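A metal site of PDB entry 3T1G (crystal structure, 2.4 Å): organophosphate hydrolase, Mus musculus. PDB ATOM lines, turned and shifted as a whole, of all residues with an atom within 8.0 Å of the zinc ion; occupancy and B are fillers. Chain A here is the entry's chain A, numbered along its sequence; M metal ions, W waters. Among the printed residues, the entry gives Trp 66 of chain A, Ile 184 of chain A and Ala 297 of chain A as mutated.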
ATOM      1  N   HIS A  16      13.060   4.963  -5.553  1.00  0.00           N
ATOM      2  CA  HIS A  16      12.187   3.801  -5.555  1.00  0.00           C
ATOM      3  C   HIS A  16      10.789   4.186  -5.093  1.00  0.00           C
ATOM      4  O   HIS A  16      10.523   4.269  -3.891  1.00  0.00           O
ATOM      5  CB  HIS A  16      12.743   2.705  -4.640  1.00  0.00           C
ATOM      6  CG  HIS A  16      12.050   1.385  -4.766  1.00  0.00           C
ATOM      7  ND1 HIS A  16      12.739   0.207  -4.978  1.00  0.00           N
ATOM      8  CD2 HIS A  16      10.740   1.042  -4.690  1.00  0.00           C
ATOM      9  CE1 HIS A  16      11.874  -0.800  -5.024  1.00  0.00           C
ATOM     10  NE2 HIS A  16      10.652  -0.316  -4.862  1.00  0.00           N
ATOM     11  N   VAL A  17       9.907   4.420  -6.064  1.00  0.00           N
ATOM     12  CA  VAL A  17       8.500   4.738  -5.792  1.00  0.00           C
ATOM     13  C   VAL A  17       7.678   4.365  -7.017  1.00  0.00           C
ATOM     14  O   VAL A  17       8.074   4.672  -8.146  1.00  0.00           O
ATOM     15  CB  VAL A  17       8.311   6.233  -5.372  1.00  0.00           C
ATOM     16  CG1 VAL A  17       9.024   7.186  -6.349  1.00  0.00           C
ATOM     17  CG2 VAL A  17       6.808   6.593  -5.222  1.00  0.00           C
ATOM     18  N   HIS A  18       6.549   3.678  -6.794  1.00  0.00           N
ATOM     19  CA  HIS A  18       5.691   3.192  -7.873  1.00  0.00           C
ATOM     20  C   HIS A  18       4.572   4.212  -8.145  1.00  0.00           C
ATOM     21  O   HIS A  18       3.800   4.574  -7.244  1.00  0.00           O
ATOM     22  CB  HIS A  18       5.088   1.816  -7.525  1.00  0.00           C
ATOM     23  CG  HIS A  18       6.104   0.742  -7.231  1.00  0.00           C
ATOM     24  ND1 HIS A  18       6.344  -0.308  -8.104  1.00  0.00           N
ATOM     25  CD2 HIS A  18       6.932   0.546  -6.184  1.00  0.00           C
ATOM     26  CE1 HIS A  18       7.275  -1.099  -7.583  1.00  0.00           C
ATOM     27  NE2 HIS A  18       7.645  -0.602  -6.414  1.00  0.00           N
ATOM     28  N   TRP A  66      -4.434  -2.944  -5.322  1.00  0.00           N
ATOM     29  CA  TRP A  66      -4.410  -2.403  -6.682  1.00  0.00           C
ATOM     30  C   TRP A  66      -5.688  -2.731  -7.486  1.00  0.00           C
ATOM     31  O   TRP A  66      -6.158  -1.912  -8.268  1.00  0.00           O
ATOM     32  CB  TRP A  66      -3.142  -2.860  -7.435  1.00  0.00           C
ATOM     33  CG  TRP A  66      -1.956  -1.943  -7.267  1.00  0.00           C
ATOM     34  CD1 TRP A  66      -1.498  -1.025  -8.172  1.00  0.00           C
ATOM     35  CD2 TRP A  66      -1.054  -1.869  -6.135  1.00  0.00           C
ATOM     36  NE1 TRP A  66      -0.390  -0.379  -7.677  1.00  0.00           N
ATOM     37  CE2 TRP A  66      -0.092  -0.875  -6.432  1.00  0.00           C
ATOM     38  CE3 TRP A  66      -0.974  -2.540  -4.906  1.00  0.00           C
ATOM     39  CZ2 TRP A  66       0.953  -0.533  -5.546  1.00  0.00           C
ATOM     40  CZ3 TRP A  66       0.071  -2.198  -4.020  1.00  0.00           C
ATOM     41  CH2 TRP A  66       1.014  -1.199  -4.349  1.00  0.00           C
ATOM     42  N   ARG A 102       8.510   4.649 -11.085  1.00  0.00           N
ATOM     43  CA  ARG A 102       8.451   3.407 -11.858  1.00  0.00           C
ATOM     44  C   ARG A 102       7.029   2.854 -11.997  1.00  0.00           C
ATOM     45  O   ARG A 102       6.157   3.085 -11.148  1.00  0.00           O
ATOM     46  CB  ARG A 102       9.372   2.336 -11.235  1.00  0.00           C
ATOM     47  CG  ARG A 102       8.928   1.816  -9.862  1.00  0.00           C
ATOM     48  CD  ARG A 102       9.981   0.908  -9.226  1.00  0.00           C
ATOM     49  NE  ARG A 102      11.216   1.617  -8.888  1.00  0.00           N
ATOM     50  CZ  ARG A 102      12.361   1.031  -8.556  1.00  0.00           C
ATOM     51  NH1 ARG A 102      12.450  -0.290  -8.503  1.00  0.00           N
ATOM     52  NH2 ARG A 102      13.409   1.766  -8.258  1.00  0.00           N
ATOM     53  N   CYS A 154       8.844  -1.262 -15.766  1.00  0.00           N
ATOM     54  CA  CYS A 154       8.902  -2.504 -14.989  1.00  0.00           C
ATOM     55  C   CYS A 154       8.557  -3.781 -15.748  1.00  0.00           C
ATOM     56  O   CYS A 154       7.492  -3.896 -16.348  1.00  0.00           O
ATOM     57  CB  CYS A 154       7.982  -2.410 -13.767  1.00  0.00           C
ATOM     58  SG  CYS A 154       8.416  -1.127 -12.596  1.00  0.00           S
ATOM     59  N   ASP A 182      13.125  -2.006 -14.573  1.00  0.00           N
ATOM     60  CA  ASP A 182      12.937  -2.656 -13.262  1.00  0.00           C
ATOM     61  C   ASP A 182      12.354  -4.045 -13.460  1.00  0.00           C
ATOM     62  O   ASP A 182      11.892  -4.396 -14.556  1.00  0.00           O
ATOM     63  CB  ASP A 182      12.015  -1.810 -12.383  1.00  0.00           C
ATOM     64  CG  ASP A 182      11.949  -2.281 -10.912  1.00  0.00           C
ATOM     65  OD1 ASP A 182      12.871  -2.949 -10.395  1.00  0.00           O
ATOM     66  OD2 ASP A 182      10.946  -1.936 -10.245  1.00  0.00           O
ATOM     67  N   LEU A 183      12.399  -4.844 -12.405  1.00  0.00           N
ATOM     68  CA  LEU A 183      11.788  -6.170 -12.384  1.00  0.00           C
ATOM     69  C   LEU A 183      11.051  -6.274 -11.053  1.00  0.00           C
ATOM     70  O   LEU A 183      11.667  -6.224  -9.989  1.00  0.00           O
ATOM     71  CB  LEU A 183      12.842  -7.278 -12.513  1.00  0.00           C
ATOM     72  CG  LEU A 183      12.363  -8.731 -12.445  1.00  0.00           C
ATOM     73  CD1 LEU A 183      11.446  -9.086 -13.617  1.00  0.00           C
ATOM     74  CD2 LEU A 183      13.520  -9.695 -12.365  1.00  0.00           C
ATOM     75  N   ILE A 184       9.712  -6.362 -11.135  1.00  0.00           N
ATOM     76  CA  ILE A 184       8.851  -6.501  -9.959  1.00  0.00           C
ATOM     77  C   ILE A 184       8.148  -7.853  -9.969  1.00  0.00           C
ATOM     78  O   ILE A 184       8.250  -8.620 -10.934  1.00  0.00           O
ATOM     79  CB  ILE A 184       7.785  -5.373  -9.845  1.00  0.00           C
ATOM     80  CG1 ILE A 184       6.874  -5.330 -11.093  1.00  0.00           C
ATOM     81  CG2 ILE A 184       8.446  -4.039  -9.587  1.00  0.00           C
ATOM     82  CD1 ILE A 184       5.744  -4.280 -11.028  1.00  0.00           C
ATOM     83  N   GLY A 185       7.423  -8.133  -8.881  1.00  0.00           N
ATOM     84  CA  GLY A 185       6.632  -9.347  -8.777  1.00  0.00           C
ATOM     85  C   GLY A 185       7.087 -10.246  -7.650  1.00  0.00           C
ATOM     86  O   GLY A 185       7.911  -9.864  -6.822  1.00  0.00           O
ATOM     87  N   HIS A 215      13.957  -5.586  -7.980  1.00  0.00           N
ATOM     88  CA  HIS A 215      13.403  -5.927  -6.652  1.00  0.00           C
ATOM     89  C   HIS A 215      13.974  -7.289  -6.245  1.00  0.00           C
ATOM     90  O   HIS A 215      13.762  -8.289  -6.933  1.00  0.00           O
ATOM     91  CB  HIS A 215      11.863  -6.026  -6.703  1.00  0.00           C
ATOM     92  CG  HIS A 215      11.136  -4.701  -6.663  1.00  0.00           C
ATOM     93  ND1 HIS A 215      11.247  -3.761  -7.656  1.00  0.00           N
ATOM     94  CD2 HIS A 215      10.228  -4.223  -5.781  1.00  0.00           C
ATOM     95  CE1 HIS A 215      10.470  -2.727  -7.370  1.00  0.00           C
ATOM     96  NE2 HIS A 215       9.835  -2.985  -6.244  1.00  0.00           N
ATOM     97  N   GLU A 218      13.638  -8.579  -0.711  1.00  0.00           N
ATOM     98  CA  GLU A 218      12.615  -7.854   0.034  1.00  0.00           C
ATOM     99  C   GLU A 218      12.062  -8.697   1.189  1.00  0.00           C
ATOM    100  O   GLU A 218      12.044  -8.231   2.310  1.00  0.00           O
ATOM    101  CB  GLU A 218      11.498  -7.346  -0.891  1.00  0.00           C
ATOM    102  CG  GLU A 218      10.503  -6.408  -0.219  1.00  0.00           C
ATOM    103  CD  GLU A 218       9.446  -5.835  -1.156  1.00  0.00           C
ATOM    104  OE1 GLU A 218       9.509  -6.090  -2.382  1.00  0.00           O
ATOM    105  OE2 GLU A 218       8.540  -5.131  -0.658  1.00  0.00           O
ATOM    106  N   GLY A 238      16.433  -3.140  -5.367  1.00  0.00           N
ATOM    107  CA  GLY A 238      15.249  -2.650  -4.679  1.00  0.00           C
ATOM    108  C   GLY A 238      15.045  -3.447  -3.418  1.00  0.00           C
ATOM    109  O   GLY A 238      14.904  -4.662  -3.472  1.00  0.00           O
ATOM    110  N   HIS A 239      15.055  -2.753  -2.278  1.00  0.00           N
ATOM    111  CA  HIS A 239      14.937  -3.352  -0.940  1.00  0.00           C
ATOM    112  C   HIS A 239      16.227  -4.029  -0.501  1.00  0.00           C
ATOM    113  O   HIS A 239      17.096  -3.367   0.054  1.00  0.00           O
ATOM    114  CB  HIS A 239      13.744  -4.319  -0.837  1.00  0.00           C
ATOM    115  CG  HIS A 239      12.442  -3.698  -1.234  1.00  0.00           C
ATOM    116  ND1 HIS A 239      11.736  -2.851  -0.399  1.00  0.00           N
ATOM    117  CD2 HIS A 239      11.693  -3.821  -2.360  1.00  0.00           C
ATOM    118  CE1 HIS A 239      10.624  -2.470  -0.996  1.00  0.00           C
ATOM    119  NE2 HIS A 239      10.573  -3.043  -2.189  1.00  0.00           N
ATOM    120  N   GLU A 261      18.091   0.268  -2.555  1.00  0.00           N
ATOM    121  CA  GLU A 261      16.955   1.170  -2.464  1.00  0.00           C
ATOM    122  C   GLU A 261      16.082   0.766  -1.278  1.00  0.00           C
ATOM    123  O   GLU A 261      15.268  -0.156  -1.382  1.00  0.00           O
ATOM    124  CB  GLU A 261      16.139   1.182  -3.770  1.00  0.00           C
ATOM    125  CG  GLU A 261      16.942   1.442  -5.053  1.00  0.00           C
ATOM    126  CD  GLU A 261      16.222   1.028  -6.329  1.00  0.00           C
ATOM    127  OE1 GLU A 261      15.061   0.551  -6.229  1.00  0.00           O
ATOM    128  OE2 GLU A 261      16.794   1.197  -7.422  1.00  0.00           O
ATOM    129  N   CYS A 263      13.238   0.937   1.675  1.00  0.00           N
ATOM    130  CA  CYS A 263      11.880   1.410   1.939  1.00  0.00           C
ATOM    131  C   CYS A 263      11.403   0.980   3.335  1.00  0.00           C
ATOM    132  O   CYS A 263      10.680  -0.015   3.481  1.00  0.00           O
ATOM    133  CB  CYS A 263      10.931   0.912   0.836  1.00  0.00           C
ATOM    134  SG  CYS A 263      11.579   1.141  -0.854  1.00  0.00           S
ATOM    135  N   SER A 266       7.561   0.910   4.256  1.00  0.00           N
ATOM    136  CA  SER A 266       7.026  -0.152   3.404  1.00  0.00           C
ATOM    137  C   SER A 266       7.314  -1.519   3.978  1.00  0.00           C
ATOM    138  O   SER A 266       6.400  -2.340   4.112  1.00  0.00           O
ATOM    139  CB  SER A 266       7.600  -0.054   1.979  1.00  0.00           C
ATOM    140  OG  SER A 266       7.382  -1.257   1.262  1.00  0.00           O
ATOM    141  N   THR A 295       9.747   5.888  -0.460  1.00  0.00           N
ATOM    142  CA  THR A 295       8.381   5.640   0.018  1.00  0.00           C
ATOM    143  C   THR A 295       7.759   4.370  -0.547  1.00  0.00           C
ATOM    144  O   THR A 295       6.880   3.794   0.091  1.00  0.00           O
ATOM    145  CB  THR A 295       7.411   6.815  -0.263  1.00  0.00           C
ATOM    146  OG1 THR A 295       7.329   7.072  -1.673  1.00  0.00           O
ATOM    147  CG2 THR A 295       7.856   8.087   0.470  1.00  0.00           C
ATOM    148  N   ASP A 296       8.197   3.960  -1.736  1.00  0.00           N
ATOM    149  CA  ASP A 296       7.682   2.737  -2.381  1.00  0.00           C
ATOM    150  C   ASP A 296       6.223   2.886  -2.909  1.00  0.00           C
ATOM    151  O   ASP A 296       6.023   3.016  -4.121  1.00  0.00           O
ATOM    152  CB  ASP A 296       7.835   1.504  -1.461  1.00  0.00           C
ATOM    153  CG  ASP A 296       7.737   0.186  -2.214  1.00  0.00           C
ATOM    154  OD1 ASP A 296       7.670   0.229  -3.460  1.00  0.00           O
ATOM    155  OD2 ASP A 296       7.740  -0.891  -1.580  1.00  0.00           O
ATOM    156  N   ALA A 297       5.233   2.882  -2.025  1.00  0.00           N
ATOM    157  CA  ALA A 297       3.829   3.033  -2.428  1.00  0.00           C
ATOM    158  C   ALA A 297       3.074   3.902  -1.405  1.00  0.00           C
ATOM    159  O   ALA A 297       2.325   3.377  -0.594  1.00  0.00           O
ATOM    160  CB  ALA A 297       3.158   1.657  -2.585  1.00  0.00           C
ATOM    161  N   PHE A 301       0.577   2.982   1.762  1.00  0.00           N
ATOM    162  CA  PHE A 301       1.257   3.102   3.045  1.00  0.00           C
ATOM    163  C   PHE A 301       0.953   4.416   3.760  1.00  0.00           C
ATOM    164  O   PHE A 301       1.515   4.693   4.813  1.00  0.00           O
ATOM    165  CB  PHE A 301       2.768   2.907   2.865  1.00  0.00           C
ATOM    166  CG  PHE A 301       3.149   1.623   2.169  1.00  0.00           C
ATOM    167  CD1 PHE A 301       2.435   0.437   2.389  1.00  0.00           C
ATOM    168  CD2 PHE A 301       4.248   1.581   1.321  1.00  0.00           C
ATOM    169  CE1 PHE A 301       2.794  -0.742   1.756  1.00  0.00           C
ATOM    170  CE2 PHE A 301       4.608   0.418   0.684  1.00  0.00           C
ATOM    171  CZ  PHE A 301       3.888  -0.757   0.897  1.00  0.00           C
HETATM  172 ZN    ZN M   1       8.789  -1.420  -4.974  1.00  0.00          ZN
HETATM  173  O   HOH W   1       7.877  -2.799  -3.474  1.00  0.00           O
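The side-chain carboxylate of Asp 296 sits at hydrogen-bond distance from the side-chain hydroxyl of Ser 266, at 2.9 Å. ND1 of His 215 lies close to OD2 of Asp 182, at 3.2 Å. O of Glu 261 sits at hydrogen-bond distance from N of His 239. A ring nitrogen (NE2) of His 239 lies close to the side-chain carboxylate (OE1) of Glu 218. ND1 of His 16 sits at hydrogen-bond distance from OE1 of Glu 261. O of Leu 183 lies within hydrogen-bond range of N of His 215.
His 239 touches the zinc ion.
The zinc ion is bound by a ring nitrogen (NE2) of His 18 (2.0 Å), a ring nitrogen (NE2) of His 16 (2.2 Å), water W1 (2.2 Å), a ring nitrogen (NE2) of His 215 (2.3 Å) and the side-chain carboxylate of Asp 296 (2.5 Å). The zinc ion has five donor atoms within binding distance.
Water W1 bridges OD2 of Asp 296 (2.7 Å) and NE2 of His 239 (3.0 Å).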
